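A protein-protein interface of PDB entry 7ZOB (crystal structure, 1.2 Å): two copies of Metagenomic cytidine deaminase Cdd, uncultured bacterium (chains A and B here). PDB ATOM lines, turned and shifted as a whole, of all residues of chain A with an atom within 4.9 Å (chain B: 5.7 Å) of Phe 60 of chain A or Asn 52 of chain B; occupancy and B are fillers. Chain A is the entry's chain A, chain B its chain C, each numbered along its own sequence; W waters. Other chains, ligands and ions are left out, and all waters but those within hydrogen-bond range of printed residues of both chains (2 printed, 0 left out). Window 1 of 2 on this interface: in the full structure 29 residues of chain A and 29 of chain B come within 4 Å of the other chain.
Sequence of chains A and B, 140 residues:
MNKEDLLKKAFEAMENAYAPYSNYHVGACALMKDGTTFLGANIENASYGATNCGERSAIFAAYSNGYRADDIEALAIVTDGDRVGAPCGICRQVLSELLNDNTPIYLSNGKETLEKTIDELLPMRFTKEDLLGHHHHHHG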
ATOM      1  N   ASN A  52       6.328 -23.918 -16.213  1.00  0.00           N
ATOM      2  CA  ASN A  52       6.606 -24.005 -17.640  1.00  0.00           C
ATOM      3  C   ASN A  52       7.014 -25.415 -18.021  1.00  0.00           C
ATOM      4  O   ASN A  52       7.731 -26.098 -17.276  1.00  0.00           O
ATOM      5  CB  ASN A  52       7.713 -23.033 -18.052  1.00  0.00           C
ATOM      6  CG  ASN A  52       7.787 -22.827 -19.571  1.00  0.00           C
ATOM      7  OD1 ASN A  52       8.849 -23.031 -20.186  1.00  0.00           O
ATOM      8  ND2 ASN A  52       6.686 -22.454 -20.185  1.00  0.00           N
ATOM      9  N   ARG A  56       8.378 -26.083 -24.119  1.00  0.00           N
ATOM     10  CA  ARG A  56       8.292 -24.627 -24.241  1.00  0.00           C
ATOM     11  C   ARG A  56       9.626 -23.973 -23.875  1.00  0.00           C
ATOM     12  O   ARG A  56      10.072 -23.041 -24.554  1.00  0.00           O
ATOM     13  CB  ARG A  56       7.136 -24.080 -23.399  1.00  0.00           C
ATOM     14  CG  ARG A  56       5.786 -24.242 -24.126  1.00  0.00           C
ATOM     15  CD  ARG A  56       4.644 -23.574 -23.378  1.00  0.00           C
ATOM     16  NE  ARG A  56       4.238 -24.375 -22.221  1.00  0.00           N
ATOM     17  CZ  ARG A  56       3.675 -23.881 -21.120  1.00  0.00           C
ATOM     18  NH1 ARG A  56       3.408 -22.583 -20.994  1.00  0.00           N
ATOM     19  NH2 ARG A  56       3.385 -24.713 -20.108  1.00  0.00           N
ATOM     20  N   SER A  57      10.263 -24.420 -22.786  1.00  0.00           N
ATOM     21  CA  SER A  57      11.583 -23.884 -22.460  1.00  0.00           C
ATOM     22  C   SER A  57      12.512 -23.928 -23.672  1.00  0.00           C
ATOM     23  O   SER A  57      13.210 -22.954 -23.974  1.00  0.00           O
ATOM     24  CB  SER A  57      12.218 -24.646 -21.300  1.00  0.00           C
ATOM     25  OG  SER A  57      11.476 -24.467 -20.093  1.00  0.00           O
ATOM     26  N   ALA A  58      12.534 -25.062 -24.370  1.00  0.00           N
ATOM     27  CA  ALA A  58      13.465 -25.238 -25.486  1.00  0.00           C
ATOM     28  C   ALA A  58      13.122 -24.329 -26.664  1.00  0.00           C
ATOM     29  O   ALA A  58      13.993 -23.650 -27.222  1.00  0.00           O
ATOM     30  CB  ALA A  58      13.435 -26.691 -25.957  1.00  0.00           C
ATOM     31  N   ILE A  59      11.847 -24.293 -27.054  1.00  0.00           N
ATOM     32  CA  ILE A  59      11.478 -23.530 -28.239  1.00  0.00           C
ATOM     33  C   ILE A  59      11.552 -22.036 -27.967  1.00  0.00           C
ATOM     34  O   ILE A  59      11.928 -21.263 -28.855  1.00  0.00           O
ATOM     35  CB  ILE A  59      10.105 -23.978 -28.788  1.00  0.00           C
ATOM     36  CG1 ILE A  59       9.922 -23.537 -30.244  1.00  0.00           C
ATOM     37  CG2 ILE A  59       8.930 -23.477 -27.937  1.00  0.00           C
ATOM     38  CD1 ILE A  59      10.810 -24.231 -31.188  1.00  0.00           C
ATOM     39  N   PHE A  60      11.220 -21.605 -26.747  1.00  0.00           N
ATOM     40  CA  PHE A  60      11.362 -20.196 -26.409  1.00  0.00           C
ATOM     41  C   PHE A  60      12.826 -19.777 -26.413  1.00  0.00           C
ATOM     42  O   PHE A  60      13.149 -18.658 -26.829  1.00  0.00           O
ATOM     43  CB  PHE A  60      10.757 -19.874 -25.045  1.00  0.00           C
ATOM     44  CG  PHE A  60       9.264 -20.060 -24.944  1.00  0.00           C
ATOM     45  CD1 PHE A  60       8.420 -19.985 -26.062  1.00  0.00           C
ATOM     46  CD2 PHE A  60       8.694 -20.317 -23.708  1.00  0.00           C
ATOM     47  CE1 PHE A  60       7.033 -20.160 -25.916  1.00  0.00           C
ATOM     48  CE2 PHE A  60       7.313 -20.468 -23.581  1.00  0.00           C
ATOM     49  CZ  PHE A  60       6.492 -20.399 -24.687  1.00  0.00           C
ATOM     50  N   ALA A  61      13.734 -20.666 -25.985  1.00  0.00           N
ATOM     51  CA  ALA A  61      15.150 -20.339 -26.058  1.00  0.00           C
ATOM     52  C   ALA A  61      15.592 -20.177 -27.503  1.00  0.00           C
ATOM     53  O   ALA A  61      16.316 -19.231 -27.835  1.00  0.00           O
ATOM     54  CB  ALA A  61      15.951 -21.452 -25.380  1.00  0.00           C
ATOM     55  N   ALA A  62      15.138 -21.068 -28.385  1.00  0.00           N
ATOM     56  CA  ALA A  62      15.527 -20.940 -29.792  1.00  0.00           C
ATOM     57  C   ALA A  62      15.060 -19.615 -30.382  1.00  0.00           C
ATOM     58  O   ALA A  62      15.839 -18.898 -31.023  1.00  0.00           O
ATOM     59  CB  ALA A  62      14.967 -22.121 -30.564  1.00  0.00           C
ATOM     60  N   TYR A  63      13.784 -19.282 -30.174  1.00  0.00           N
ATOM     61  CA  TYR A  63      13.242 -18.044 -30.724  1.00  0.00           C
ATOM     62  C   TYR A  63      13.917 -16.827 -30.116  1.00  0.00           C
ATOM     63  O   TYR A  63      14.137 -15.822 -30.810  1.00  0.00           O
ATOM     64  CB  TYR A  63      11.732 -17.994 -30.500  1.00  0.00           C
ATOM     65  CG  TYR A  63      10.933 -18.581 -31.635  1.00  0.00           C
ATOM     66  CD1 TYR A  63      10.971 -19.931 -31.938  1.00  0.00           C
ATOM     67  CD2 TYR A  63      10.115 -17.755 -32.435  1.00  0.00           C
ATOM     68  CE1 TYR A  63      10.260 -20.456 -33.006  1.00  0.00           C
ATOM     69  CE2 TYR A  63       9.384 -18.285 -33.474  1.00  0.00           C
ATOM     70  CZ  TYR A  63       9.469 -19.615 -33.774  1.00  0.00           C
ATOM     71  OH  TYR A  63       8.742 -20.112 -34.833  1.00  0.00           O
ATOM     72  N   SER A  64      14.270 -16.899 -28.828  1.00  0.00           N
ATOM     73  CA  SER A  64      14.902 -15.761 -28.165  1.00  0.00           C
ATOM     74  C   SER A  64      16.298 -15.493 -28.694  1.00  0.00           C
ATOM     75  O   SER A  64      16.837 -14.394 -28.479  1.00  0.00           O
ATOM     76  CB  SER A  64      15.008 -16.021 -26.668  1.00  0.00           C
ATOM     77  OG  SER A  64      13.733 -16.054 -26.058  1.00  0.00           O
ATOM     78  N   VAL A  94       1.353 -23.682 -28.463  1.00  0.00           N
ATOM     79  CA  VAL A  94       2.597 -22.982 -28.782  1.00  0.00           C
ATOM     80  C   VAL A  94       3.245 -23.554 -30.039  1.00  0.00           C
ATOM     81  O   VAL A  94       3.616 -22.804 -30.961  1.00  0.00           O
ATOM     82  CB  VAL A  94       3.544 -22.990 -27.569  1.00  0.00           C
ATOM     83  CG1 VAL A  94       4.929 -22.490 -27.984  1.00  0.00           C
ATOM     84  CG2 VAL A  94       2.946 -22.132 -26.457  1.00  0.00           C
ATOM     85  N   LEU A  98       4.717 -22.019 -33.611  1.00  0.00           N
ATOM     86  CA  LEU A  98       6.156 -21.817 -33.719  1.00  0.00           C
ATOM     87  C   LEU A  98       6.883 -22.864 -34.551  1.00  0.00           C
ATOM     88  O   LEU A  98       8.054 -22.643 -34.896  1.00  0.00           O
ATOM     89  CB  LEU A  98       6.783 -21.722 -32.324  1.00  0.00           C
ATOM     90  CG  LEU A  98       6.244 -20.650 -31.379  1.00  0.00           C
ATOM     91  CD1 LEU A  98       7.077 -20.618 -30.139  1.00  0.00           C
ATOM     92  CD2 LEU A  98       6.236 -19.287 -32.037  1.00  0.00           C
ATOM     93  N   ALA B  41      13.398 -13.313 -25.057  1.00  0.00           N
ATOM     94  CA  ALA B  41      12.534 -12.318 -25.657  1.00  0.00           C
ATOM     95  C   ALA B  41      11.091 -12.800 -25.526  1.00  0.00           C
ATOM     96  O   ALA B  41      10.826 -13.992 -25.323  1.00  0.00           O
ATOM     97  CB  ALA B  41      12.923 -12.097 -27.122  1.00  0.00           C
ATOM     98  N   ASN B  42      10.153 -11.857 -25.610  1.00  0.00           N
ATOM     99  CA  ASN B  42       8.749 -12.239 -25.543  1.00  0.00           C
ATOM    100  C   ASN B  42       8.329 -12.960 -26.812  1.00  0.00           C
ATOM    101  O   ASN B  42       8.799 -12.650 -27.917  1.00  0.00           O
ATOM    102  CB  ASN B  42       7.823 -11.072 -25.208  1.00  0.00           C
ATOM    103  CG  ASN B  42       7.934  -9.911 -26.170  1.00  0.00           C
ATOM    104  OD1 ASN B  42       9.043  -9.489 -26.544  1.00  0.00           O
ATOM    105  ND2 ASN B  42       6.796  -9.351 -26.550  1.00  0.00           N
ATOM    106  N   ILE B  43       7.446 -13.944 -26.660  1.00  0.00           N
ATOM    107  CA  ILE B  43       7.022 -14.804 -27.760  1.00  0.00           C
ATOM    108  C   ILE B  43       5.516 -14.996 -27.650  1.00  0.00           C
ATOM    109  O   ILE B  43       5.026 -15.751 -26.799  1.00  0.00           O
ATOM    110  CB  ILE B  43       7.756 -16.146 -27.750  1.00  0.00           C
ATOM    111  CG1 ILE B  43       9.271 -15.944 -27.862  1.00  0.00           C
ATOM    112  CG2 ILE B  43       7.299 -17.005 -28.918  1.00  0.00           C
ATOM    113  CD1 ILE B  43      10.076 -17.128 -27.348  1.00  0.00           C
ATOM    114  N   GLU B  44       4.785 -14.284 -28.497  1.00  0.00           N
ATOM    115  CA  GLU B  44       3.338 -14.268 -28.482  1.00  0.00           C
ATOM    116  C   GLU B  44       2.741 -15.481 -29.188  1.00  0.00           C
ATOM    117  O   GLU B  44       3.433 -16.237 -29.877  1.00  0.00           O
ATOM    118  CB  GLU B  44       2.790 -12.962 -29.038  1.00  0.00           C
ATOM    119  CG  GLU B  44       3.271 -11.785 -28.226  1.00  0.00           C
ATOM    120  CD  GLU B  44       2.764 -10.434 -28.667  1.00  0.00           C
ATOM    121  OE1 GLU B  44       2.280 -10.261 -29.823  1.00  0.00           O
ATOM    122  OE2 GLU B  44       2.863  -9.515 -27.805  1.00  0.00           O
ATOM    123  N   ALA B  50      -1.171 -18.126 -24.159  1.00  0.00           N
ATOM    124  CA  ALA B  50       0.025 -18.938 -24.347  1.00  0.00           C
ATOM    125  C   ALA B  50       1.283 -18.094 -24.561  1.00  0.00           C
ATOM    126  O   ALA B  50       2.375 -18.658 -24.741  1.00  0.00           O
ATOM    127  CB  ALA B  50      -0.181 -19.911 -25.514  1.00  0.00           C
ATOM    128  N   THR B  51       1.164 -16.767 -24.566  1.00  0.00           N
ATOM    129  CA  THR B  51       2.313 -15.871 -24.710  1.00  0.00           C
ATOM    130  C   THR B  51       3.292 -16.067 -23.560  1.00  0.00           C
ATOM    131  O   THR B  51       2.894 -16.236 -22.403  1.00  0.00           O
ATOM    132  CB  THR B  51       1.802 -14.425 -24.712  1.00  0.00           C
ATOM    133  OG1 THR B  51       1.009 -14.233 -25.888  1.00  0.00           O
ATOM    134  CG2 THR B  51       2.913 -13.398 -24.647  1.00  0.00           C
ATOM    135  N   ASN B  52       4.591 -16.002 -23.866  1.00  0.00           N
ATOM    136  CA  ASN B  52       5.633 -16.014 -22.846  1.00  0.00           C
ATOM    137  C   ASN B  52       6.384 -14.691 -22.828  1.00  0.00           C
ATOM    138  O   ASN B  52       6.663 -14.103 -23.888  1.00  0.00           O
ATOM    139  CB  ASN B  52       6.627 -17.149 -23.086  1.00  0.00           C
ATOM    140  CG  ASN B  52       7.506 -17.435 -21.869  1.00  0.00           C
ATOM    141  OD1 ASN B  52       8.751 -17.414 -21.963  1.00  0.00           O
ATOM    142  ND2 ASN B  52       6.895 -17.665 -20.731  1.00  0.00           N
ATOM    143  N   CYS B  53       6.759 -14.250 -21.648  1.00  0.00           N
ATOM    144  CA  CYS B  53       7.511 -13.022 -21.484  1.00  0.00           C
ATOM    145  C   CYS B  53       9.006 -13.269 -21.663  1.00  0.00           C
ATOM    146  O   CYS B  53       9.525 -14.370 -21.432  1.00  0.00           O
ATOM    147  CB  CYS B  53       7.276 -12.481 -20.063  1.00  0.00           C
ATOM    148  SG  CYS B  53       5.565 -11.912 -19.782  1.00  0.00           S
ATOM    149  N   GLY B  54       9.715 -12.210 -22.051  1.00  0.00           N
ATOM    150  CA  GLY B  54      11.139 -12.349 -22.319  1.00  0.00           C
ATOM    151  C   GLY B  54      11.976 -12.739 -21.112  1.00  0.00           C
ATOM    152  O   GLY B  54      12.916 -13.536 -21.224  1.00  0.00           O
ATOM    153  N   ARG B  56      11.033 -14.506 -18.597  1.00  0.00           N
ATOM    154  CA  ARG B  56      10.813 -15.935 -18.394  1.00  0.00           C
ATOM    155  C   ARG B  56      11.592 -16.760 -19.418  1.00  0.00           C
ATOM    156  O   ARG B  56      12.191 -17.782 -19.066  1.00  0.00           O
ATOM    157  CB  ARG B  56       9.315 -16.245 -18.416  1.00  0.00           C
ATOM    158  CG  ARG B  56       8.646 -15.971 -17.049  1.00  0.00           C
ATOM    159  CD  ARG B  56       7.190 -16.404 -17.002  1.00  0.00           C
ATOM    160  NE  ARG B  56       6.344 -15.489 -17.773  1.00  0.00           N
ATOM    161  CZ  ARG B  56       5.183 -15.836 -18.333  1.00  0.00           C
ATOM    162  NH1 ARG B  56       4.707 -17.074 -18.232  1.00  0.00           N
ATOM    163  NH2 ARG B  56       4.502 -14.926 -19.046  1.00  0.00           N
ATOM    164  N   SER B  57      11.571 -16.359 -20.694  1.00  0.00           N
ATOM    165  CA  SER B  57      12.380 -17.076 -21.680  1.00  0.00           C
ATOM    166  C   SER B  57      13.824 -17.218 -21.212  1.00  0.00           C
ATOM    167  O   SER B  57      14.410 -18.301 -21.299  1.00  0.00           O
ATOM    168  CB  SER B  57      12.351 -16.380 -23.036  1.00  0.00           C
ATOM    169  OG  SER B  57      11.037 -16.383 -23.596  1.00  0.00           O
ATOM    170  N   PHE B  60      14.162 -19.469 -17.841  1.00  0.00           N
ATOM    171  CA  PHE B  60      13.883 -20.872 -18.129  1.00  0.00           C
ATOM    172  C   PHE B  60      15.014 -21.504 -18.928  1.00  0.00           C
ATOM    173  O   PHE B  60      15.353 -22.679 -18.710  1.00  0.00           O
ATOM    174  CB  PHE B  60      12.575 -21.035 -18.894  1.00  0.00           C
ATOM    175  CG  PHE B  60      11.331 -20.614 -18.145  1.00  0.00           C
ATOM    176  CD1 PHE B  60      11.265 -20.621 -16.739  1.00  0.00           C
ATOM    177  CD2 PHE B  60      10.200 -20.231 -18.859  1.00  0.00           C
ATOM    178  CE1 PHE B  60      10.079 -20.250 -16.089  1.00  0.00           C
ATOM    179  CE2 PHE B  60       9.028 -19.872 -18.198  1.00  0.00           C
ATOM    180  CZ  PHE B  60       8.977 -19.881 -16.813  1.00  0.00           C
HETATM  181  O   HOH W   1       3.567 -20.354 -22.794  1.00  0.00           O
HETATM  182  O   HOH W   2      12.843 -20.532 -22.317  1.00  0.00           O
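The side-chain hydroxyl of Ser 64 of chain A lies within hydrogen-bond range of the backbone NH of Ala 41 of chain B, 2.9 Å away.
O of Phe 60 of chain A lies within hydrogen-bond range of OG of Ser 64 of chain A, 2.8 Å away.
The backbone NH (N) of Ile 43 of chain B sits at hydrogen-bond distance from the backbone carbonyl oxygen (O) of Asn 52 of chain B, at 2.9 Å.
The backbone carbonyl oxygen (O) of Ala 41 of chain B is in hydrogen-bond range of the side-chain hydroxyl (OG) of Ser 57 of chain B, 3.0 Å away.
The guanidinium group of Arg 56 of chain A sits close to the side-chain amide nitrogen of Asn 52 of chain A, 3.4 Å away.
OG of Ser 57 of chain B lies within hydrogen-bond range of OD1 of Asn 52 of chain B, 3.0 Å away.
OD1 of Asn 52 of chain A sits at hydrogen-bond distance from OG of Ser 57 of chain A, at 3.0 Å.
Among the printed residues, pairs that only touch across the chains: Ser 64 of chain A with Ser 57 of chain B, Asn 52 of chain A with Phe 60 of chain B, Phe 60 of chain A with Asn 52 of chain B, Phe 60 of chain A with Ile 43 of chain B, Tyr 63 of chain A with Ile 43 of chain B, Phe 60 of chain A with Ser 57 of chain B, Ser 57 of chain A with Phe 60 of chain B, Leu 98 of chain A with Ile 43 of chain B and Val 94 of chain A with Ala 50 of chain B.
Of the printed residues of chain B, Phe 60 of chain A touches Ile 43 (3.5 Å), Asn 52 (3.4 Å) and Ser 57 (3.8 Å).
Of chain A, only Phe 60 (3.4 Å) comes within 4 Å of Asn 52 of chain B.
Printed residues of chain A within 4 Å of Ser 57 of chain B: Phe 60 (3.8 Å) and Ser 64 (3.3 Å).
Of the printed residues of chain A, Ala 50 of chain B touches Val 94.
Of the printed residues of chain A, Phe 60 of chain B touches Asn 52 and Ser 57.
Of the printed residues of chain B, Asn 52 of chain A touches Phe 60.
Cys 53 of chain B touches none of the printed residues of chain A.
Ala 58 of chain A touches none of the printed residues of chain B.
The nearest residue of chain A that does not touch Asn 52 of chain B is Asn 52 of chain A (4.8 Å).
Of the 12 printed residues of chain A, 7 touch a printed residue of chain B.
Hydrophobic or aromatic side chains of chain A within 4 Å of the printed part of chain B: Phe 60, Tyr 63, Val 94 and Leu 98.
Of the 12 printed residues of chain B, 6 touch a printed residue of chain A.
Among the printed residues, 10 pairs touch across the chains.
Among the printed residues, no Asp or Glu carboxylate lies within 4 Å of a Lys or Arg side-chain nitrogen of the other chain.
Asn 52 of chain A touches Phe 60 of chain B, and with the chains exchanged Phe 60 of chain A touches Asn 52 of chain B.
Ser 57 of chain A touches Phe 60 of chain B, and with the chains exchanged Phe 60 of chain A touches Ser 57 of chain B.
Positions printed for both chains: 52, 56, 57 and 60.
Of the 10 pairs that touch across the chains among the printed residues, 4 have their exchanged pair printed and touching as well.
Water W1 lies within hydrogen-bond range of O of Ala 50 of chain B (2.8 Å) and NH1 of Arg 56 of chain A (2.9 Å).
Water W2 lies within hydrogen-bond range of O of Ser 57 of chain B (2.9 Å) and O of Ser 57 of chain A (3.0 Å).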
